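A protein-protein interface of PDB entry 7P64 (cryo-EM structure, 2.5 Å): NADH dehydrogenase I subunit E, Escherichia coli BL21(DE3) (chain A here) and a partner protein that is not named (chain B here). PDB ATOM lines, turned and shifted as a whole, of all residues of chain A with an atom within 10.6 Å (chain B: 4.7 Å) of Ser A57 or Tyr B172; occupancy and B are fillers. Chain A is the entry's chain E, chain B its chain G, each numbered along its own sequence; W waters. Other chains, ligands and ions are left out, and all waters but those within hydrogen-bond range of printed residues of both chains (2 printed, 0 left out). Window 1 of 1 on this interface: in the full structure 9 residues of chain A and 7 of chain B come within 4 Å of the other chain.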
ATOM      1  N   ARG A  23      16.666  14.967 -26.921  1.00  0.00           N
ATOM      2  CA  ARG A  23      15.311  14.430 -26.829  1.00  0.00           C
ATOM      3  C   ARG A  23      14.262  15.517 -27.018  1.00  0.00           C
ATOM      4  O   ARG A  23      13.155  15.238 -27.493  1.00  0.00           O
ATOM      5  CB  ARG A  23      15.120  13.734 -25.480  1.00  0.00           C
ATOM      6  CG  ARG A  23      13.809  12.983 -25.337  1.00  0.00           C
ATOM      7  CD  ARG A  23      13.417  12.832 -23.886  1.00  0.00           C
ATOM      8  NE  ARG A  23      14.345  11.967 -23.173  1.00  0.00           N
ATOM      9  CZ  ARG A  23      14.279  10.644 -23.164  1.00  0.00           C
ATOM     10  NH1 ARG A  23      13.328   9.996 -23.815  1.00  0.00           N
ATOM     11  NH2 ARG A  23      15.188   9.954 -22.484  1.00  0.00           N
ATOM     12  N   SER A  26      12.140  15.997 -30.359  1.00  0.00           N
ATOM     13  CA  SER A  26      11.350  14.883 -30.876  1.00  0.00           C
ATOM     14  C   SER A  26      10.043  15.354 -31.497  1.00  0.00           C
ATOM     15  O   SER A  26       9.652  14.874 -32.568  1.00  0.00           O
ATOM     16  CB  SER A  26      11.079  13.872 -29.763  1.00  0.00           C
ATOM     17  OG  SER A  26      10.338  14.459 -28.712  1.00  0.00           O
ATOM     18  N   LEU A  30       9.138  15.005 -35.451  1.00  0.00           N
ATOM     19  CA  LEU A  30       7.908  14.386 -35.927  1.00  0.00           C
ATOM     20  C   LEU A  30       7.105  15.351 -36.788  1.00  0.00           C
ATOM     21  O   LEU A  30       6.537  14.953 -37.810  1.00  0.00           O
ATOM     22  CB  LEU A  30       7.072  13.902 -34.745  1.00  0.00           C
ATOM     23  CG  LEU A  30       7.569  12.663 -34.004  1.00  0.00           C
ATOM     24  CD1 LEU A  30       6.919  12.579 -32.641  1.00  0.00           C
ATOM     25  CD2 LEU A  30       7.288  11.411 -34.804  1.00  0.00           C
ATOM     26  N   ASP A  42       5.599   4.299 -40.239  1.00  0.00           N
ATOM     27  CA  ASP A  42       6.095   3.442 -39.167  1.00  0.00           C
ATOM     28  C   ASP A  42       7.616   3.479 -39.060  1.00  0.00           C
ATOM     29  O   ASP A  42       8.163   3.475 -37.951  1.00  0.00           O
ATOM     30  CB  ASP A  42       5.608   2.010 -39.380  1.00  0.00           C
ATOM     31  CG  ASP A  42       4.134   1.847 -39.078  1.00  0.00           C
ATOM     32  OD1 ASP A  42       3.407   2.861 -39.094  1.00  0.00           O
ATOM     33  OD2 ASP A  42       3.699   0.704 -38.826  1.00  0.00           O
ATOM     34  N   ALA A  44       9.485   5.975 -39.816  1.00  0.00           N
ATOM     35  CA  ALA A  44       9.909   7.302 -39.391  1.00  0.00           C
ATOM     36  C   ALA A  44      10.176   7.358 -37.895  1.00  0.00           C
ATOM     37  O   ALA A  44      11.032   8.129 -37.454  1.00  0.00           O
ATOM     38  CB  ALA A  44       8.861   8.340 -39.781  1.00  0.00           C
ATOM     39  N   ILE A  45       9.464   6.548 -37.108  1.00  0.00           N
ATOM     40  CA  ILE A  45       9.690   6.502 -35.666  1.00  0.00           C
ATOM     41  C   ILE A  45      11.097   6.000 -35.367  1.00  0.00           C
ATOM     42  O   ILE A  45      11.841   6.608 -34.586  1.00  0.00           O
ATOM     43  CB  ILE A  45       8.622   5.623 -34.992  1.00  0.00           C
ATOM     44  CG1 ILE A  45       7.227   6.187 -35.263  1.00  0.00           C
ATOM     45  CG2 ILE A  45       8.885   5.500 -33.503  1.00  0.00           C
ATOM     46  CD1 ILE A  45       6.962   7.512 -34.596  1.00  0.00           C
ATOM     47  N   HIS A  46      11.497   4.906 -36.018  1.00  0.00           N
ATOM     48  CA  HIS A  46      12.833   4.365 -35.804  1.00  0.00           C
ATOM     49  C   HIS A  46      13.906   5.281 -36.377  1.00  0.00           C
ATOM     50  O   HIS A  46      14.986   5.407 -35.794  1.00  0.00           O
ATOM     51  CB  HIS A  46      12.941   2.966 -36.408  1.00  0.00           C
ATOM     52  CG  HIS A  46      14.082   2.165 -35.862  1.00  0.00           C
ATOM     53  ND1 HIS A  46      15.302   2.080 -36.497  1.00  0.00           N
ATOM     54  CD2 HIS A  46      14.191   1.422 -34.736  1.00  0.00           C
ATOM     55  CE1 HIS A  46      16.112   1.314 -35.789  1.00  0.00           C
ATOM     56  NE2 HIS A  46      15.462   0.902 -34.715  1.00  0.00           N
ATOM     57  N   ALA A  47      13.624   5.938 -37.508  1.00  0.00           N
ATOM     58  CA  ALA A  47      14.597   6.870 -38.079  1.00  0.00           C
ATOM     59  C   ALA A  47      14.826   8.077 -37.171  1.00  0.00           C
ATOM     60  O   ALA A  47      15.975   8.480 -36.940  1.00  0.00           O
ATOM     61  CB  ALA A  47      14.140   7.318 -39.464  1.00  0.00           C
ATOM     62  N   ILE A  48      13.746   8.660 -36.643  1.00  0.00           N
ATOM     63  CA  ILE A  48      13.861   9.793 -35.731  1.00  0.00           C
ATOM     64  C   ILE A  48      14.554   9.372 -34.442  1.00  0.00           C
ATOM     65  O   ILE A  48      15.378  10.114 -33.894  1.00  0.00           O
ATOM     66  CB  ILE A  48      12.466  10.397 -35.474  1.00  0.00           C
ATOM     67  CG1 ILE A  48      11.994  11.177 -36.700  1.00  0.00           C
ATOM     68  CG2 ILE A  48      12.453  11.311 -34.258  1.00  0.00           C
ATOM     69  CD1 ILE A  48      10.534  11.538 -36.652  1.00  0.00           C
ATOM     70  N   ALA A  49      14.254   8.164 -33.952  1.00  0.00           N
ATOM     71  CA  ALA A  49      14.917   7.655 -32.758  1.00  0.00           C
ATOM     72  C   ALA A  49      16.411   7.455 -32.986  1.00  0.00           C
ATOM     73  O   ALA A  49      17.223   7.736 -32.099  1.00  0.00           O
ATOM     74  CB  ALA A  49      14.264   6.347 -32.325  1.00  0.00           C
ATOM     75  N   ASP A  50      16.787   6.960 -34.167  1.00  0.00           N
ATOM     76  CA  ASP A  50      18.198   6.766 -34.484  1.00  0.00           C
ATOM     77  C   ASP A  50      18.931   8.095 -34.600  1.00  0.00           C
ATOM     78  O   ASP A  50      20.090   8.205 -34.185  1.00  0.00           O
ATOM     79  CB  ASP A  50      18.339   5.967 -35.777  1.00  0.00           C
ATOM     80  CG  ASP A  50      18.170   4.479 -35.563  1.00  0.00           C
ATOM     81  OD1 ASP A  50      18.091   4.051 -34.393  1.00  0.00           O
ATOM     82  OD2 ASP A  50      18.114   3.738 -36.567  1.00  0.00           O
ATOM     83  N   GLY A  53      18.997   9.690 -30.857  1.00  0.00           N
ATOM     84  CA  GLY A  53      19.633   8.948 -29.789  1.00  0.00           C
ATOM     85  C   GLY A  53      18.724   8.606 -28.631  1.00  0.00           C
ATOM     86  O   GLY A  53      19.191   8.518 -27.491  1.00  0.00           O
ATOM     87  N   ILE A  54      17.438   8.419 -28.888  1.00  0.00           N
ATOM     88  CA  ILE A  54      16.477   8.027 -27.861  1.00  0.00           C
ATOM     89  C   ILE A  54      15.814   6.742 -28.334  1.00  0.00           C
ATOM     90  O   ILE A  54      15.888   6.399 -29.526  1.00  0.00           O
ATOM     91  CB  ILE A  54      15.451   9.149 -27.575  1.00  0.00           C
ATOM     92  CG1 ILE A  54      14.709   9.555 -28.846  1.00  0.00           C
ATOM     93  CG2 ILE A  54      16.131  10.348 -26.931  1.00  0.00           C
ATOM     94  CD1 ILE A  54      13.646  10.590 -28.596  1.00  0.00           C
ATOM     95  N   PRO A  55      15.215   5.967 -27.425  1.00  0.00           N
ATOM     96  CA  PRO A  55      14.492   4.763 -27.853  1.00  0.00           C
ATOM     97  C   PRO A  55      13.299   5.086 -28.741  1.00  0.00           C
ATOM     98  O   PRO A  55      12.682   6.147 -28.633  1.00  0.00           O
ATOM     99  CB  PRO A  55      14.041   4.132 -26.532  1.00  0.00           C
ATOM    100  CG  PRO A  55      15.011   4.612 -25.541  1.00  0.00           C
ATOM    101  CD  PRO A  55      15.406   5.988 -25.962  1.00  0.00           C
ATOM    102  N   ALA A  56      12.986   4.143 -29.634  1.00  0.00           N
ATOM    103  CA  ALA A  56      11.831   4.281 -30.512  1.00  0.00           C
ATOM    104  C   ALA A  56      10.514   4.241 -29.753  1.00  0.00           C
ATOM    105  O   ALA A  56       9.518   4.779 -30.245  1.00  0.00           O
ATOM    106  CB  ALA A  56      11.847   3.187 -31.579  1.00  0.00           C
ATOM    107  N   SER A  57      10.485   3.612 -28.576  1.00  0.00           N
ATOM    108  CA  SER A  57       9.271   3.615 -27.769  1.00  0.00           C
ATOM    109  C   SER A  57       8.954   5.013 -27.254  1.00  0.00           C
ATOM    110  O   SER A  57       7.781   5.389 -27.156  1.00  0.00           O
ATOM    111  CB  SER A  57       9.406   2.624 -26.613  1.00  0.00           C
ATOM    112  OG  SER A  57      10.603   2.835 -25.891  1.00  0.00           O
ATOM    113  N   ASP A  58       9.983   5.804 -26.940  1.00  0.00           N
ATOM    114  CA  ASP A  58       9.762   7.189 -26.534  1.00  0.00           C
ATOM    115  C   ASP A  58       9.199   8.025 -27.679  1.00  0.00           C
ATOM    116  O   ASP A  58       8.274   8.824 -27.475  1.00  0.00           O
ATOM    117  CB  ASP A  58      11.064   7.798 -26.016  1.00  0.00           C
ATOM    118  CG  ASP A  58      11.461   7.250 -24.660  1.00  0.00           C
ATOM    119  OD1 ASP A  58      10.570   7.062 -23.806  1.00  0.00           O
ATOM    120  OD2 ASP A  58      12.667   7.013 -24.445  1.00  0.00           O
ATOM    121  N   VAL A  59       9.733   7.842 -28.889  1.00  0.00           N
ATOM    122  CA  VAL A  59       9.229   8.564 -30.055  1.00  0.00           C
ATOM    123  C   VAL A  59       7.797   8.154 -30.360  1.00  0.00           C
ATOM    124  O   VAL A  59       6.958   8.991 -30.707  1.00  0.00           O
ATOM    125  CB  VAL A  59      10.149   8.336 -31.269  1.00  0.00           C
ATOM    126  CG1 VAL A  59       9.749   9.241 -32.417  1.00  0.00           C
ATOM    127  CG2 VAL A  59      11.589   8.576 -30.891  1.00  0.00           C
ATOM    128  N   GLU A  60       7.492   6.861 -30.235  1.00  0.00           N
ATOM    129  CA  GLU A  60       6.133   6.394 -30.487  1.00  0.00           C
ATOM    130  C   GLU A  60       5.161   6.910 -29.432  1.00  0.00           C
ATOM    131  O   GLU A  60       4.024   7.266 -29.756  1.00  0.00           O
ATOM    132  CB  GLU A  60       6.107   4.869 -30.555  1.00  0.00           C
ATOM    133  CG  GLU A  60       4.747   4.277 -30.889  1.00  0.00           C
ATOM    134  CD  GLU A  60       4.290   4.603 -32.297  1.00  0.00           C
ATOM    135  OE1 GLU A  60       5.152   4.805 -33.172  1.00  0.00           O
ATOM    136  OE2 GLU A  60       3.068   4.649 -32.533  1.00  0.00           O
ATOM    137  N   GLY A  61       5.593   6.966 -28.170  1.00  0.00           N
ATOM    138  CA  GLY A  61       4.745   7.527 -27.130  1.00  0.00           C
ATOM    139  C   GLY A  61       4.467   9.001 -27.339  1.00  0.00           C
ATOM    140  O   GLY A  61       3.343   9.465 -27.128  1.00  0.00           O
ATOM    141  N   VAL A  62       5.480   9.751 -27.776  1.00  0.00           N
ATOM    142  CA  VAL A  62       5.276  11.160 -28.101  1.00  0.00           C
ATOM    143  C   VAL A  62       4.342  11.310 -29.299  1.00  0.00           C
ATOM    144  O   VAL A  62       3.416  12.127 -29.277  1.00  0.00           O
ATOM    145  CB  VAL A  62       6.633  11.848 -28.336  1.00  0.00           C
ATOM    146  CG1 VAL A  62       6.450  13.196 -28.997  1.00  0.00           C
ATOM    147  CG2 VAL A  62       7.367  12.010 -27.023  1.00  0.00           C
ATOM    148  N   ALA A  63       4.545  10.506 -30.346  1.00  0.00           N
ATOM    149  CA  ALA A  63       3.745  10.633 -31.562  1.00  0.00           C
ATOM    150  C   ALA A  63       2.286  10.268 -31.321  1.00  0.00           C
ATOM    151  O   ALA A  63       1.383  10.909 -31.868  1.00  0.00           O
ATOM    152  CB  ALA A  63       4.335   9.764 -32.670  1.00  0.00           C
ATOM    153  N   THR A  64       2.031   9.244 -30.510  1.00  0.00           N
ATOM    154  CA  THR A  64       0.661   8.864 -30.206  1.00  0.00           C
ATOM    155  C   THR A  64       0.044   9.703 -29.097  1.00  0.00           C
ATOM    156  O   THR A  64      -1.177   9.662 -28.926  1.00  0.00           O
ATOM    157  CB  THR A  64       0.594   7.389 -29.823  1.00  0.00           C
ATOM    158  OG1 THR A  64       1.600   7.107 -28.845  1.00  0.00           O
ATOM    159  CG2 THR A  64       0.820   6.518 -31.037  1.00  0.00           C
ATOM    160  N   PHE A  65       0.846  10.449 -28.336  1.00  0.00           N
ATOM    161  CA  PHE A  65       0.269  11.338 -27.335  1.00  0.00           C
ATOM    162  C   PHE A  65      -0.385  12.552 -27.979  1.00  0.00           C
ATOM    163  O   PHE A  65      -1.497  12.937 -27.601  1.00  0.00           O
ATOM    164  CB  PHE A  65       1.337  11.778 -26.337  1.00  0.00           C
ATOM    165  CG  PHE A  65       0.793  12.559 -25.180  1.00  0.00           C
ATOM    166  CD1 PHE A  65       0.237  11.911 -24.095  1.00  0.00           C
ATOM    167  CD2 PHE A  65       0.830  13.942 -25.180  1.00  0.00           C
ATOM    168  CE1 PHE A  65      -0.266  12.623 -23.031  1.00  0.00           C
ATOM    169  CE2 PHE A  65       0.325  14.657 -24.122  1.00  0.00           C
ATOM    170  CZ  PHE A  65      -0.222  13.998 -23.045  1.00  0.00           C
ATOM    171  N   TYR A  66       0.281  13.168 -28.949  1.00  0.00           N
ATOM    172  CA  TYR A  66      -0.170  14.433 -29.509  1.00  0.00           C
ATOM    173  C   TYR A  66      -1.080  14.187 -30.702  1.00  0.00           C
ATOM    174  O   TYR A  66      -0.734  13.429 -31.613  1.00  0.00           O
ATOM    175  CB  TYR A  66       1.026  15.297 -29.906  1.00  0.00           C
ATOM    176  CG  TYR A  66       1.849  15.716 -28.717  1.00  0.00           C
ATOM    177  CD1 TYR A  66       1.430  16.739 -27.884  1.00  0.00           C
ATOM    178  CD2 TYR A  66       3.033  15.069 -28.411  1.00  0.00           C
ATOM    179  CE1 TYR A  66       2.175  17.112 -26.792  1.00  0.00           C
ATOM    180  CE2 TYR A  66       3.781  15.432 -27.320  1.00  0.00           C
ATOM    181  CZ  TYR A  66       3.349  16.456 -26.514  1.00  0.00           C
ATOM    182  OH  TYR A  66       4.096  16.823 -25.424  1.00  0.00           O
ATOM    183  N   ARG A  71      -0.283   9.382 -37.088  1.00  0.00           N
ATOM    184  CA  ARG A  71       0.362   8.086 -37.228  1.00  0.00           C
ATOM    185  C   ARG A  71      -0.412   7.156 -38.150  1.00  0.00           C
ATOM    186  O   ARG A  71      -0.063   5.978 -38.264  1.00  0.00           O
ATOM    187  CB  ARG A  71       0.548   7.446 -35.854  1.00  0.00           C
ATOM    188  CG  ARG A  71       1.745   7.982 -35.093  1.00  0.00           C
ATOM    189  CD  ARG A  71       3.037   7.635 -35.800  1.00  0.00           C
ATOM    190  NE  ARG A  71       3.434   6.261 -35.525  1.00  0.00           N
ATOM    191  CZ  ARG A  71       3.417   5.285 -36.420  1.00  0.00           C
ATOM    192  NH1 ARG A  71       3.056   5.503 -37.673  1.00  0.00           N
ATOM    193  NH2 ARG A  71       3.766   4.058 -36.048  1.00  0.00           N
ATOM    194  N   THR B 167      14.467  -0.511 -23.250  1.00  0.00           N
ATOM    195  CA  THR B 167      14.119   0.545 -24.186  1.00  0.00           C
ATOM    196  C   THR B 167      12.918   0.246 -25.067  1.00  0.00           C
ATOM    197  O   THR B 167      12.365   1.182 -25.651  1.00  0.00           O
ATOM    198  CB  THR B 167      15.310   0.873 -25.101  1.00  0.00           C
ATOM    199  OG1 THR B 167      15.726  -0.309 -25.794  1.00  0.00           O
ATOM    200  CG2 THR B 167      16.478   1.428 -24.295  1.00  0.00           C
ATOM    201  N   ASP B 168      12.493  -1.010 -25.181  1.00  0.00           N
ATOM    202  CA  ASP B 168      11.472  -1.389 -26.146  1.00  0.00           C
ATOM    203  C   ASP B 168      10.070  -1.448 -25.554  1.00  0.00           C
ATOM    204  O   ASP B 168       9.140  -1.860 -26.247  1.00  0.00           O
ATOM    205  CB  ASP B 168      11.818  -2.734 -26.783  1.00  0.00           C
ATOM    206  CG  ASP B 168      12.175  -3.785 -25.761  1.00  0.00           C
ATOM    207  OD1 ASP B 168      12.809  -3.442 -24.747  1.00  0.00           O
ATOM    208  OD2 ASP B 168      11.814  -4.957 -25.971  1.00  0.00           O
ATOM    209  N   LEU B 169       9.892  -1.058 -24.299  1.00  0.00           N
ATOM    210  CA  LEU B 169       8.572  -0.981 -23.694  1.00  0.00           C
ATOM    211  C   LEU B 169       8.250   0.468 -23.366  1.00  0.00           C
ATOM    212  O   LEU B 169       9.120   1.223 -22.928  1.00  0.00           O
ATOM    213  CB  LEU B 169       8.480  -1.835 -22.431  1.00  0.00           C
ATOM    214  CG  LEU B 169       7.079  -2.185 -21.932  1.00  0.00           C
ATOM    215  CD1 LEU B 169       6.576  -3.450 -22.592  1.00  0.00           C
ATOM    216  CD2 LEU B 169       7.070  -2.331 -20.426  1.00  0.00           C
ATOM    217  N   GLY B 170       6.998   0.851 -23.582  1.00  0.00           N
ATOM    218  CA  GLY B 170       6.593   2.220 -23.347  1.00  0.00           C
ATOM    219  C   GLY B 170       5.090   2.341 -23.248  1.00  0.00           C
ATOM    220  O   GLY B 170       4.344   1.369 -23.402  1.00  0.00           O
ATOM    221  N   VAL B 171       4.658   3.568 -22.975  1.00  0.00           N
ATOM    222  CA  VAL B 171       3.250   3.925 -22.899  1.00  0.00           C
ATOM    223  C   VAL B 171       2.930   4.820 -24.088  1.00  0.00           C
ATOM    224  O   VAL B 171       3.685   5.748 -24.401  1.00  0.00           O
ATOM    225  CB  VAL B 171       2.908   4.598 -21.554  1.00  0.00           C
ATOM    226  CG1 VAL B 171       3.904   5.693 -21.205  1.00  0.00           C
ATOM    227  CG2 VAL B 171       1.485   5.124 -21.544  1.00  0.00           C
ATOM    228  N   TYR B 172       1.841   4.506 -24.777  1.00  0.00           N
ATOM    229  CA  TYR B 172       1.437   5.184 -25.994  1.00  0.00           C
ATOM    230  C   TYR B 172      -0.001   5.642 -25.856  1.00  0.00           C
ATOM    231  O   TYR B 172      -0.764   5.130 -25.037  1.00  0.00           O
ATOM    232  CB  TYR B 172       1.579   4.272 -27.215  1.00  0.00           C
ATOM    233  CG  TYR B 172       2.814   3.434 -27.138  1.00  0.00           C
ATOM    234  CD1 TYR B 172       4.061   3.992 -27.366  1.00  0.00           C
ATOM    235  CD2 TYR B 172       2.746   2.098 -26.789  1.00  0.00           C
ATOM    236  CE1 TYR B 172       5.198   3.242 -27.275  1.00  0.00           C
ATOM    237  CE2 TYR B 172       3.878   1.340 -26.695  1.00  0.00           C
ATOM    238  CZ  TYR B 172       5.100   1.916 -26.939  1.00  0.00           C
ATOM    239  OH  TYR B 172       6.237   1.164 -26.842  1.00  0.00           O
ATOM    240  N   GLY B 173      -0.357   6.626 -26.661  1.00  0.00           N
ATOM    241  CA  GLY B 173      -1.719   7.091 -26.674  1.00  0.00           C
ATOM    242  C   GLY B 173      -2.002   8.177 -25.667  1.00  0.00           C
ATOM    243  O   GLY B 173      -1.132   8.980 -25.325  1.00  0.00           O
ATOM    244  N   ALA B 174      -3.225   8.176 -25.161  1.00  0.00           N
ATOM    245  CA  ALA B 174      -3.815   9.352 -24.547  1.00  0.00           C
ATOM    246  C   ALA B 174      -4.796   8.943 -23.460  1.00  0.00           C
ATOM    247  O   ALA B 174      -4.678   7.857 -22.888  1.00  0.00           O
ATOM    248  CB  ALA B 174      -4.494  10.226 -25.601  1.00  0.00           C
ATOM    249  N   ASN B 177      -7.182   5.778 -23.621  1.00  0.00           N
ATOM    250  CA  ASN B 177      -6.616   4.848 -24.582  1.00  0.00           C
ATOM    251  C   ASN B 177      -5.121   4.647 -24.368  1.00  0.00           C
ATOM    252  O   ASN B 177      -4.383   4.429 -25.333  1.00  0.00           O
ATOM    253  CB  ASN B 177      -6.889   5.337 -26.001  1.00  0.00           C
ATOM    254  CG  ASN B 177      -7.246   4.217 -26.943  1.00  0.00           C
ATOM    255  OD1 ASN B 177      -7.894   3.250 -26.553  1.00  0.00           O
ATOM    256  ND2 ASN B 177      -6.818   4.334 -28.190  1.00  0.00           N
ATOM    257  N   VAL B 178      -4.656   4.742 -23.122  1.00  0.00           N
ATOM    258  CA  VAL B 178      -3.250   4.500 -22.824  1.00  0.00           C
ATOM    259  C   VAL B 178      -2.933   3.030 -23.047  1.00  0.00           C
ATOM    260  O   VAL B 178      -3.600   2.141 -22.504  1.00  0.00           O
ATOM    261  CB  VAL B 178      -2.911   4.926 -21.387  1.00  0.00           C
ATOM    262  CG1 VAL B 178      -2.283   6.304 -21.374  1.00  0.00           C
ATOM    263  CG2 VAL B 178      -4.145   4.885 -20.505  1.00  0.00           C
ATOM    264  N   TYR B 179      -1.911   2.770 -23.851  1.00  0.00           N
ATOM    265  CA  TYR B 179      -1.499   1.427 -24.222  1.00  0.00           C
ATOM    266  C   TYR B 179      -0.091   1.190 -23.706  1.00  0.00           C
ATOM    267  O   TYR B 179       0.799   2.009 -23.931  1.00  0.00           O
ATOM    268  CB  TYR B 179      -1.551   1.253 -25.739  1.00  0.00           C
ATOM    269  CG  TYR B 179      -1.510  -0.176 -26.210  1.00  0.00           C
ATOM    270  CD1 TYR B 179      -0.302  -0.813 -26.447  1.00  0.00           C
ATOM    271  CD2 TYR B 179      -2.680  -0.883 -26.432  1.00  0.00           C
ATOM    272  CE1 TYR B 179      -0.261  -2.115 -26.880  1.00  0.00           C
ATOM    273  CE2 TYR B 179      -2.648  -2.182 -26.867  1.00  0.00           C
ATOM    274  CZ  TYR B 179      -1.436  -2.794 -27.089  1.00  0.00           C
ATOM    275  OH  TYR B 179      -1.397  -4.092 -27.524  1.00  0.00           O
ATOM    276  N   GLY B 181       3.070  -1.268 -23.919  1.00  0.00           N
ATOM    277  CA  GLY B 181       3.625  -2.364 -24.689  1.00  0.00           C
ATOM    278  C   GLY B 181       4.802  -1.911 -25.524  1.00  0.00           C
ATOM    279  O   GLY B 181       5.454  -0.919 -25.215  1.00  0.00           O
ATOM    280  N   ARG B 182       5.071  -2.665 -26.560  1.00  0.00           N
ATOM    281  CA  ARG B 182       6.136  -2.368 -27.501  1.00  0.00           C
ATOM    282  C   ARG B 182       5.606  -1.521 -28.647  1.00  0.00           C
ATOM    283  O   ARG B 182       4.404  -1.524 -28.923  1.00  0.00           O
ATOM    284  CB  ARG B 182       6.731  -3.669 -28.032  1.00  0.00           C
ATOM    285  CG  ARG B 182       7.371  -4.545 -26.985  1.00  0.00           C
ATOM    286  CD  ARG B 182       8.099  -5.713 -27.624  1.00  0.00           C
ATOM    287  NE  ARG B 182       9.467  -5.377 -27.996  1.00  0.00           N
ATOM    288  CZ  ARG B 182       9.888  -5.217 -29.242  1.00  0.00           C
ATOM    289  NH1 ARG B 182       9.069  -5.348 -30.270  1.00  0.00           N
ATOM    290  NH2 ARG B 182      11.164  -4.921 -29.461  1.00  0.00           N
ATOM    291  N   PRO B 183       6.471  -0.760 -29.335  1.00  0.00           N
ATOM    292  CA  PRO B 183       6.003  -0.038 -30.530  1.00  0.00           C
ATOM    293  C   PRO B 183       5.578  -0.952 -31.667  1.00  0.00           C
ATOM    294  O   PRO B 183       4.812  -0.518 -32.534  1.00  0.00           O
ATOM    295  CB  PRO B 183       7.212   0.822 -30.923  1.00  0.00           C
ATOM    296  CG  PRO B 183       8.372   0.159 -30.302  1.00  0.00           C
ATOM    297  CD  PRO B 183       7.883  -0.459 -29.038  1.00  0.00           C
HETATM  298  O   HOH W   1       6.511   6.030 -24.283  1.00  0.00           O
HETATM  299  O   HOH W   2      12.288   1.005 -28.476  1.00  0.00           O
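Printed residues of chain B that touch a printed residue of chain A: Thr B167, Leu B169, Val B171, Tyr B172 and Gly B173.
Hydrophobic or aromatic side chains of chain B within 4 Å of the printed part of chain A: Tyr B172.
Of the 26 printed residues of chain A, 6 touch a printed residue of chain B.
Hydrophobic or aromatic side chains of chain A within 4 Å of the printed part of chain B: Pro A55 and Phe A65.
Among the printed residues, no Asp or Glu carboxylate lies within 4 Å of a Lys or Arg side-chain nitrogen of the other chain.
The side-chain hydroxyl (OG) of Ser A57 sits at hydrogen-bond distance from the backbone carbonyl oxygen (O) of Thr B167 (2.4 Å).
OG1 of Thr A64 is in hydrogen-bond range of N of Gly B173 (3.0 Å).
Water W2 lies within hydrogen-bond range of O of Thr B167 (2.8 Å), N of Ser A57 (3.2 Å) and N of Ala A56 (3.4 Å).
Water W1 lies within hydrogen-bond range of the backbone carbonyl oxygen (O) of Val B171 (2.8 Å) and the backbone carbonyl oxygen (O) of Ser A57 (3.2 Å).
Among the printed residues, merely in contact across the chains: Thr A64 with Tyr B172, Ser A57 with Tyr B172, Phe A65 with Gly B173, Gly A61 with Val B171, Gly A61 with Tyr B172, Pro A55 with Thr B167, Glu A60 with Tyr B172 and Ser A57 with Leu B169.
The backbone carbonyl oxygen of Gly A61 lies within hydrogen-bond range of the side-chain hydroxyl of Thr A64.
OE1 of Glu A60 is in salt-bridge range of NE of Arg A71 (3.3 Å).
The backbone NH of Tyr B172 sits at hydrogen-bond distance from the backbone carbonyl oxygen of Tyr B179 (2.8 Å).
The side-chain hydroxyl of Tyr B172 lies within hydrogen-bond range of the backbone carbonyl oxygen of Gly B181 (2.8 Å).
OH of Tyr B172 sits at hydrogen-bond distance from N of Gly B170 (3.4 Å).
The side-chain hydroxyl of Thr A64 sits at hydrogen-bond distance from the backbone carbonyl oxygen of Glu A60 (2.6 Å).
Arg A23 touches none of the printed residues of chain B.
Of the printed residues of chain B, Pro A55 touches Thr B167.
Ser A57 touches just these residues of chain B: Thr B167 (2.4 Å), Leu B169 (3.7 Å) and Tyr B172 (3.4 Å).
Of the printed residues of chain B, Gly A61 touches Val B171 and Tyr B172.
Of the printed residues of chain B, Thr A64 touches Tyr B172 and Gly B173.
Printed residues of chain B within 4 Å of Phe A65: Gly B173.
Of the printed residues of chain A, Thr B167 touches Pro A55 (3.5 Å) and Ser A57 (2.4 Å).
No residue of chain A comes within 4 Å of Gly B170.
Val B171 touches just one residue of chain A: Gly A61 (3.4 Å).
Printed residues of chain A within 4 Å of Tyr B172: Ser A57, Glu A60, Gly A61 and Thr A64.
Of chain A, only Thr A64 (3.0 Å) and Phe A65 (3.4 Å) come within 4 Å of Gly B173.
No residue of chain A comes within 4 Å of Ala B174.
No residue of chain A comes within 4 Å of Val B178.
No residue of chain A comes within 4 Å of Gly B181.
No residue of chain A comes within 4 Å of Pro B183.
The nearest printed residue of chain B that does not touch Thr A64 is Ala B174 (4.5 Å).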
